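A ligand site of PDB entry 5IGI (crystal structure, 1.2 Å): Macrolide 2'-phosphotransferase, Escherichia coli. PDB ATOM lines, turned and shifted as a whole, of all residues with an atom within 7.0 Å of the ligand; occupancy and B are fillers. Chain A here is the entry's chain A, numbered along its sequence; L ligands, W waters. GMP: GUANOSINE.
The side-chain carboxylate of Asp 219 sits at hydrogen-bond distance from an oxygen (O3') of the ligand, at 2.6 Å. N7 of the ligand lies within hydrogen-bond range of OH of Tyr 94. The backbone carbonyl oxygen of Asp 99 is in hydrogen-bond range of a nitrogen (N2) of the ligand (2.8 Å). O of Leu 97 lies within hydrogen-bond range of N1 of the ligand, 2.7 Å away. N of Leu 97 is in hydrogen-bond range of O6 of the ligand, at 3.0 Å.
The backbone NH (N) of Asn 30 is in hydrogen-bond range of the backbone carbonyl oxygen (O) of Ile 38 (2.8 Å). The side-chain carboxylate of Asp 219 lies within hydrogen-bond range of a ring nitrogen (NE2) of His 205 (2.9 Å). O of Tyr 94 sits at hydrogen-bond distance from N of Val 50 (2.8 Å). N of Ile 218 sits at hydrogen-bond distance from O of His 205 (2.9 Å).
Ile 38 touches the ligand. Val 50 touches the ligand (CG2 to N7, 3.6 Å). CE of Met 96 touches N2 of the ligand (3.7 Å). His 205 touches the ligand (CD2 to O3', 3.6 Å). Leu 207 touches the ligand (CD2 to N2, 3.8 Å). CD1 of Ile 218 touches C2' of the ligand, 3.4 Å away. Of the 23 residues printed, 10 come within 4 Å of the ligand.
Water W6 bridges O2' of the ligand (2.7 Å) and O of Gly 204 (2.8 Å). Water W3 lies within hydrogen-bond range of an oxygen (O5') of the ligand (2.8 Å), the guanidinium group of Arg 52 (2.9 Å) and the side-chain hydroxyl of Tyr 94 (3.0 Å). Water W7 lies within hydrogen-bond range of N2 of the ligand and N of Thr 101. Water W4 lies within hydrogen-bond range of OH of Tyr 202 (2.5 Å), NE2 of His 205 (3.3 Å) and O3' of the ligand (3.4 Å). Water W1 lies within hydrogen-bond range of NE2 of His 205 and O3' of the ligand.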
ATOM      1  N   ASN A  30       0.351   1.453 -27.871  1.00  0.00           N
ATOM      2  CA  ASN A  30       0.827   2.732 -27.369  1.00  0.00           C
ATOM      3  C   ASN A  30       1.477   3.518 -28.489  1.00  0.00           C
ATOM      4  O   ASN A  30       2.518   3.133 -29.020  1.00  0.00           O
ATOM      5  CB  ASN A  30       1.811   2.533 -26.234  1.00  0.00           C
ATOM      6  CG  ASN A  30       2.343   3.849 -25.677  1.00  0.00           C
ATOM      7  OD1 ASN A  30       2.314   4.878 -26.345  1.00  0.00           O
ATOM      8  ND2 ASN A  30       2.836   3.810 -24.444  1.00  0.00           N
ATOM      9  N   ILE A  38       4.292   1.000 -30.107  1.00  0.00           N
ATOM     10  CA  ILE A  38       4.583  -0.179 -29.304  1.00  0.00           C
ATOM     11  C   ILE A  38       3.271  -0.936 -29.088  1.00  0.00           C
ATOM     12  O   ILE A  38       2.305  -0.387 -28.542  1.00  0.00           O
ATOM     13  CB  ILE A  38       5.199   0.200 -27.952  1.00  0.00           C
ATOM     14  CG1 ILE A  38       6.434   1.091 -28.112  1.00  0.00           C
ATOM     15  CG2 ILE A  38       5.561  -1.068 -27.184  1.00  0.00           C
ATOM     16  CD1 ILE A  38       7.568   0.436 -28.849  1.00  0.00           C
ATOM     17  N   ILE A  40       1.602  -4.623 -27.678  1.00  0.00           N
ATOM     18  CA  ILE A  40       1.752  -5.926 -27.044  1.00  0.00           C
ATOM     19  C   ILE A  40       0.632  -6.787 -27.581  1.00  0.00           C
ATOM     20  O   ILE A  40      -0.555  -6.463 -27.407  1.00  0.00           O
ATOM     21  CB  ILE A  40       1.785  -5.829 -25.517  1.00  0.00           C
ATOM     22  CG1 ILE A  40       2.964  -4.956 -25.085  1.00  0.00           C
ATOM     23  CG2 ILE A  40       1.884  -7.239 -24.915  1.00  0.00           C
ATOM     24  CD1 ILE A  40       3.161  -4.853 -23.576  1.00  0.00           C
ATOM     25  N   VAL A  50       6.106  -8.242 -27.824  1.00  0.00           N
ATOM     26  CA  VAL A  50       6.149  -6.797 -28.023  1.00  0.00           C
ATOM     27  C   VAL A  50       6.543  -6.523 -29.458  1.00  0.00           C
ATOM     28  O   VAL A  50       7.546  -7.052 -29.953  1.00  0.00           O
ATOM     29  CB  VAL A  50       7.183  -6.141 -27.076  1.00  0.00           C
ATOM     30  CG1 VAL A  50       7.248  -4.637 -27.342  1.00  0.00           C
ATOM     31  CG2 VAL A  50       6.825  -6.437 -25.652  1.00  0.00           C
ATOM     32  N   ARG A  52       7.714  -3.553 -31.723  1.00  0.00           N
ATOM     33  CA  ARG A  52       8.343  -2.246 -31.604  1.00  0.00           C
ATOM     34  C   ARG A  52       8.484  -1.755 -33.045  1.00  0.00           C
ATOM     35  O   ARG A  52       9.344  -2.231 -33.786  1.00  0.00           O
ATOM     36  CB  ARG A  52       9.667  -2.468 -30.881  1.00  0.00           C
ATOM     37  CG  ARG A  52      10.596  -1.316 -30.798  1.00  0.00           C
ATOM     38  CD  ARG A  52      11.879  -1.730 -30.068  1.00  0.00           C
ATOM     39  NE  ARG A  52      12.796  -0.604 -29.927  1.00  0.00           N
ATOM     40  CZ  ARG A  52      12.659   0.349 -29.009  1.00  0.00           C
ATOM     41  NH1 ARG A  52      11.653   0.301 -28.144  1.00  0.00           N
ATOM     42  NH2 ARG A  52      13.531   1.341 -28.955  1.00  0.00           N
ATOM     43  N   PRO A  82      15.428  -7.656 -23.666  1.00  0.00           N
ATOM     44  CA  PRO A  82      14.624  -8.083 -24.822  1.00  0.00           C
ATOM     45  C   PRO A  82      15.414  -8.946 -25.791  1.00  0.00           C
ATOM     46  O   PRO A  82      16.554  -8.624 -26.136  1.00  0.00           O
ATOM     47  CB  PRO A  82      14.213  -6.755 -25.450  1.00  0.00           C
ATOM     48  CG  PRO A  82      14.104  -5.815 -24.276  1.00  0.00           C
ATOM     49  CD  PRO A  82      15.294  -6.217 -23.421  1.00  0.00           C
ATOM     50  N   TYR A  94       9.932  -9.042 -29.958  1.00  0.00           N
ATOM     51  CA  TYR A  94      10.530  -9.901 -28.952  1.00  0.00           C
ATOM     52  C   TYR A  94       9.441 -10.469 -28.056  1.00  0.00           C
ATOM     53  O   TYR A  94       8.449  -9.814 -27.787  1.00  0.00           O
ATOM     54  CB  TYR A  94      11.566  -9.145 -28.109  1.00  0.00           C
ATOM     55  CG  TYR A  94      11.168  -7.854 -27.418  1.00  0.00           C
ATOM     56  CD1 TYR A  94      11.293  -6.637 -28.068  1.00  0.00           C
ATOM     57  CD2 TYR A  94      10.731  -7.832 -26.100  1.00  0.00           C
ATOM     58  CE1 TYR A  94      11.009  -5.457 -27.433  1.00  0.00           C
ATOM     59  CE2 TYR A  94      10.440  -6.635 -25.478  1.00  0.00           C
ATOM     60  CZ  TYR A  94      10.571  -5.462 -26.151  1.00  0.00           C
ATOM     61  OH  TYR A  94      10.304  -4.251 -25.547  1.00  0.00           O
ATOM     62  N   PRO A  95       9.649 -11.689 -27.542  1.00  0.00           N
ATOM     63  CA  PRO A  95       8.703 -12.209 -26.566  1.00  0.00           C
ATOM     64  C   PRO A  95       8.627 -11.255 -25.369  1.00  0.00           C
ATOM     65  O   PRO A  95       9.641 -10.775 -24.878  1.00  0.00           O
ATOM     66  CB  PRO A  95       9.327 -13.559 -26.154  1.00  0.00           C
ATOM     67  CG  PRO A  95      10.306 -13.910 -27.210  1.00  0.00           C
ATOM     68  CD  PRO A  95      10.745 -12.635 -27.850  1.00  0.00           C
ATOM     69  N   MET A  96       7.424 -10.953 -24.908  1.00  0.00           N
ATOM     70  CA  MET A  96       7.287 -10.031 -23.787  1.00  0.00           C
ATOM     71  C   MET A  96       7.933 -10.617 -22.557  1.00  0.00           C
ATOM     72  O   MET A  96       7.786 -11.789 -22.244  1.00  0.00           O
ATOM     73  CB  MET A  96       5.820  -9.729 -23.470  1.00  0.00           C
ATOM     74  CG  MET A  96       5.682  -8.627 -22.418  1.00  0.00           C
ATOM     75  SD  MET A  96       4.021  -8.513 -21.772  1.00  0.00           S
ATOM     76  CE  MET A  96       4.225  -7.198 -20.582  1.00  0.00           C
ATOM     77  N   LEU A  97       8.672  -9.786 -21.858  1.00  0.00           N
ATOM     78  CA  LEU A  97       9.206 -10.127 -20.537  1.00  0.00           C
ATOM     79  C   LEU A  97       8.066  -9.780 -19.589  1.00  0.00           C
ATOM     80  O   LEU A  97       7.762  -8.602 -19.386  1.00  0.00           O
ATOM     81  CB  LEU A  97      10.482  -9.330 -20.239  1.00  0.00           C
ATOM     82  CG  LEU A  97      11.613  -9.572 -21.239  1.00  0.00           C
ATOM     83  CD1 LEU A  97      12.783  -8.626 -20.996  1.00  0.00           C
ATOM     84  CD2 LEU A  97      12.099 -11.024 -21.197  1.00  0.00           C
ATOM     85  N   GLU A  98       7.387 -10.790 -19.080  1.00  0.00           N
ATOM     86  CA  GLU A  98       6.092 -10.552 -18.446  1.00  0.00           C
ATOM     87  C   GLU A  98       6.178  -9.904 -17.086  1.00  0.00           C
ATOM     88  O   GLU A  98       5.176  -9.403 -16.575  1.00  0.00           O
ATOM     89  CB  GLU A  98       5.286 -11.844 -18.384  1.00  0.00           C
ATOM     90  CG  GLU A  98       4.828 -12.344 -19.747  1.00  0.00           C
ATOM     91  CD  GLU A  98       3.672 -11.523 -20.303  1.00  0.00           C
ATOM     92  OE1 GLU A  98       3.279 -10.531 -19.632  1.00  0.00           O
ATOM     93  OE2 GLU A  98       3.134 -11.856 -21.388  1.00  0.00           O
ATOM     94  N   ASP A  99       7.336  -9.937 -16.448  1.00  0.00           N
ATOM     95  CA  ASP A  99       7.465  -9.295 -15.146  1.00  0.00           C
ATOM     96  C   ASP A  99       7.120  -7.813 -15.279  1.00  0.00           C
ATOM     97  O   ASP A  99       7.420  -7.172 -16.291  1.00  0.00           O
ATOM     98  CB  ASP A  99       8.894  -9.428 -14.603  1.00  0.00           C
ATOM     99  CG  ASP A  99       9.178 -10.793 -14.018  1.00  0.00           C
ATOM    100  OD1 ASP A  99       8.275 -11.659 -13.959  1.00  0.00           O
ATOM    101  OD2 ASP A  99      10.336 -10.998 -13.593  1.00  0.00           O
ATOM    102  N   SER A 100       6.527  -7.258 -14.235  1.00  0.00           N
ATOM    103  CA  SER A 100       6.164  -5.864 -14.223  1.00  0.00           C
ATOM    104  C   SER A 100       7.381  -4.957 -14.249  1.00  0.00           C
ATOM    105  O   SER A 100       8.428  -5.259 -13.681  1.00  0.00           O
ATOM    106  CB  SER A 100       5.393  -5.579 -12.928  1.00  0.00           C
ATOM    107  OG  SER A 100       4.900  -4.250 -12.871  1.00  0.00           O
ATOM    108  N   THR A 101       7.191  -3.775 -14.830  1.00  0.00           N
ATOM    109  CA  THR A 101       8.095  -2.667 -14.579  1.00  0.00           C
ATOM    110  C   THR A 101       8.008  -2.255 -13.100  1.00  0.00           C
ATOM    111  O   THR A 101       7.006  -2.519 -12.396  1.00  0.00           O
ATOM    112  CB  THR A 101       7.768  -1.498 -15.508  1.00  0.00           C
ATOM    113  OG1 THR A 101       6.365  -1.218 -15.455  1.00  0.00           O
ATOM    114  CG2 THR A 101       8.121  -1.841 -16.941  1.00  0.00           C
ATOM    115  N   MET A 103       7.725   0.692 -12.021  1.00  0.00           N
ATOM    116  CA  MET A 103       6.793   1.829 -11.977  1.00  0.00           C
ATOM    117  C   MET A 103       5.678   1.512 -12.962  1.00  0.00           C
ATOM    118  O   MET A 103       5.967   1.132 -14.108  1.00  0.00           O
ATOM    119  CB  MET A 103       7.508   3.131 -12.388  1.00  0.00           C
ATOM    120  CG  MET A 103       6.617   4.405 -12.421  1.00  0.00           C
ATOM    121  SD  MET A 103       5.661   4.656 -13.945  1.00  0.00           S
ATOM    122  CE  MET A 103       6.933   4.617 -15.207  1.00  0.00           C
ATOM    123  N   ILE A 105       2.112   3.018 -14.786  1.00  0.00           N
ATOM    124  CA  ILE A 105       1.461   4.281 -15.093  1.00  0.00           C
ATOM    125  C   ILE A 105       0.530   4.065 -16.273  1.00  0.00           C
ATOM    126  O   ILE A 105       0.844   3.316 -17.190  1.00  0.00           O
ATOM    127  CB  ILE A 105       2.514   5.380 -15.381  1.00  0.00           C
ATOM    128  CG1 ILE A 105       1.858   6.753 -15.524  1.00  0.00           C
ATOM    129  CG2 ILE A 105       3.342   5.047 -16.623  1.00  0.00           C
ATOM    130  CD1 ILE A 105       2.839   7.914 -15.482  1.00  0.00           C
ATOM    131  N   TYR A 202      15.670   4.157 -15.420  1.00  0.00           N
ATOM    132  CA  TYR A 202      14.816   4.570 -14.293  1.00  0.00           C
ATOM    133  C   TYR A 202      13.855   3.433 -14.022  1.00  0.00           C
ATOM    134  O   TYR A 202      13.829   2.449 -14.752  1.00  0.00           O
ATOM    135  CB  TYR A 202      14.108   5.890 -14.593  1.00  0.00           C
ATOM    136  CG  TYR A 202      12.832   5.795 -15.402  1.00  0.00           C
ATOM    137  CD1 TYR A 202      12.819   5.349 -16.703  1.00  0.00           C
ATOM    138  CD2 TYR A 202      11.623   6.165 -14.841  1.00  0.00           C
ATOM    139  CE1 TYR A 202      11.640   5.276 -17.429  1.00  0.00           C
ATOM    140  CE2 TYR A 202      10.453   6.095 -15.569  1.00  0.00           C
ATOM    141  CZ  TYR A 202      10.473   5.662 -16.846  1.00  0.00           C
ATOM    142  OH  TYR A 202       9.265   5.621 -17.522  1.00  0.00           O
ATOM    143  N   GLY A 204      10.846   2.857 -14.585  1.00  0.00           N
ATOM    144  CA  GLY A 204       9.973   2.431 -15.669  1.00  0.00           C
ATOM    145  C   GLY A 204      10.651   1.544 -16.698  1.00  0.00           C
ATOM    146  O   GLY A 204       9.960   0.959 -17.539  1.00  0.00           O
ATOM    147  N   HIS A 205      11.972   1.445 -16.652  1.00  0.00           N
ATOM    148  CA  HIS A 205      12.718   0.587 -17.573  1.00  0.00           C
ATOM    149  C   HIS A 205      13.372  -0.601 -16.869  1.00  0.00           C
ATOM    150  O   HIS A 205      14.179  -1.302 -17.461  1.00  0.00           O
ATOM    151  CB  HIS A 205      13.767   1.394 -18.347  1.00  0.00           C
ATOM    152  CG  HIS A 205      13.162   2.340 -19.329  1.00  0.00           C
ATOM    153  ND1 HIS A 205      13.865   3.397 -19.863  1.00  0.00           N
ATOM    154  CD2 HIS A 205      11.923   2.395 -19.876  1.00  0.00           C
ATOM    155  CE1 HIS A 205      13.093   4.058 -20.706  1.00  0.00           C
ATOM    156  NE2 HIS A 205      11.913   3.473 -20.734  1.00  0.00           N
ATOM    157  N   VAL A 206      13.019  -0.815 -15.608  1.00  0.00           N
ATOM    158  CA  VAL A 206      13.513  -1.933 -14.820  1.00  0.00           C
ATOM    159  C   VAL A 206      12.350  -2.892 -14.565  1.00  0.00           C
ATOM    160  O   VAL A 206      11.249  -2.457 -14.200  1.00  0.00           O
ATOM    161  CB  VAL A 206      14.080  -1.454 -13.471  1.00  0.00           C
ATOM    162  CG1 VAL A 206      14.491  -2.640 -12.614  1.00  0.00           C
ATOM    163  CG2 VAL A 206      15.270  -0.522 -13.684  1.00  0.00           C
ATOM    164  N   LEU A 207      12.564  -4.187 -14.791  1.00  0.00           N
ATOM    165  CA  LEU A 207      11.553  -5.196 -14.487  1.00  0.00           C
ATOM    166  C   LEU A 207      11.868  -5.874 -13.184  1.00  0.00           C
ATOM    167  O   LEU A 207      13.053  -6.054 -12.850  1.00  0.00           O
ATOM    168  CB  LEU A 207      11.500  -6.259 -15.589  1.00  0.00           C
ATOM    169  CG  LEU A 207      11.342  -5.742 -17.007  1.00  0.00           C
ATOM    170  CD1 LEU A 207      11.139  -6.897 -17.993  1.00  0.00           C
ATOM    171  CD2 LEU A 207      10.212  -4.734 -17.111  1.00  0.00           C
ATOM    172  N   ILE A 218      14.705  -2.971 -19.831  1.00  0.00           N
ATOM    173  CA  ILE A 218      14.180  -2.790 -21.172  1.00  0.00           C
ATOM    174  C   ILE A 218      14.561  -1.409 -21.701  1.00  0.00           C
ATOM    175  O   ILE A 218      15.104  -0.571 -20.972  1.00  0.00           O
ATOM    176  CB  ILE A 218      12.642  -2.956 -21.189  1.00  0.00           C
ATOM    177  CG1 ILE A 218      11.953  -1.950 -20.256  1.00  0.00           C
ATOM    178  CG2 ILE A 218      12.251  -4.385 -20.814  1.00  0.00           C
ATOM    179  CD1 ILE A 218      10.413  -1.947 -20.402  1.00  0.00           C
ATOM    180  N   ASP A 219      14.282  -1.183 -22.976  1.00  0.00           N
ATOM    181  CA  ASP A 219      14.392   0.126 -23.623  1.00  0.00           C
ATOM    182  C   ASP A 219      15.843   0.633 -23.622  1.00  0.00           C
ATOM    183  O   ASP A 219      16.188   1.648 -22.992  1.00  0.00           O
ATOM    184  CB  ASP A 219      13.426   1.140 -23.019  1.00  0.00           C
ATOM    185  CG  ASP A 219      11.975   0.815 -23.275  1.00  0.00           C
ATOM    186  OD1 ASP A 219      11.632  -0.004 -24.134  1.00  0.00           O
ATOM    187  OD2 ASP A 219      11.113   1.425 -22.614  1.00  0.00           O
HETATM  188  O5' GMP L   1       9.047  -0.188 -24.930  1.00  0.00           O
HETATM  189  C5' GMP L   1       8.104   0.811 -24.534  1.00  0.00           C
HETATM  190  C4' GMP L   1       7.404   0.519 -23.211  1.00  0.00           C
HETATM  191  O4' GMP L   1       6.567  -0.671 -23.311  1.00  0.00           O
HETATM  192  C3' GMP L   1       8.298   0.240 -22.003  1.00  0.00           C
HETATM  193  O3' GMP L   1       8.845   1.405 -21.427  1.00  0.00           O
HETATM  194  C2' GMP L   1       7.369  -0.539 -21.088  1.00  0.00           C
HETATM  195  O2' GMP L   1       6.376   0.295 -20.495  1.00  0.00           O
HETATM  196  C1' GMP L   1       6.658  -1.411 -22.093  1.00  0.00           C
HETATM  197  N9  GMP L   1       7.407  -2.653 -22.376  1.00  0.00           N
HETATM  198  C8  GMP L   1       8.095  -2.879 -23.536  1.00  0.00           C
HETATM  199  N7  GMP L   1       8.633  -4.106 -23.508  1.00  0.00           N
HETATM  200  C5  GMP L   1       8.280  -4.668 -22.298  1.00  0.00           C
HETATM  201  C6  GMP L   1       8.507  -5.933 -21.705  1.00  0.00           C
HETATM  202  O6  GMP L   1       9.181  -6.903 -22.322  1.00  0.00           O
HETATM  203  N1  GMP L   1       8.030  -6.180 -20.468  1.00  0.00           N
HETATM  204  C2  GMP L   1       7.255  -5.221 -19.791  1.00  0.00           C
HETATM  205  N2  GMP L   1       6.820  -5.600 -18.534  1.00  0.00           N
HETATM  206  N3  GMP L   1       6.976  -3.983 -20.318  1.00  0.00           N
HETATM  207  C4  GMP L   1       7.501  -3.752 -21.548  1.00  0.00           C
HETATM  208  O   HOH W   1       9.786   4.651 -22.120  1.00  0.00           O
HETATM  209  O   HOH W   2       4.804  -2.569 -19.295  1.00  0.00           O
HETATM  210  O   HOH W   3       9.817  -1.764 -27.132  1.00  0.00           O
HETATM  211  O   HOH W   4       8.918   4.171 -19.530  1.00  0.00           O
HETATM  212  O   HOH W   5       3.796   0.376 -24.266  1.00  0.00           O
HETATM  213  O   HOH W   6       7.440   1.652 -18.480  1.00  0.00           O
HETATM  214  O   HOH W   7       4.870  -4.090 -16.956  1.00  0.00           O
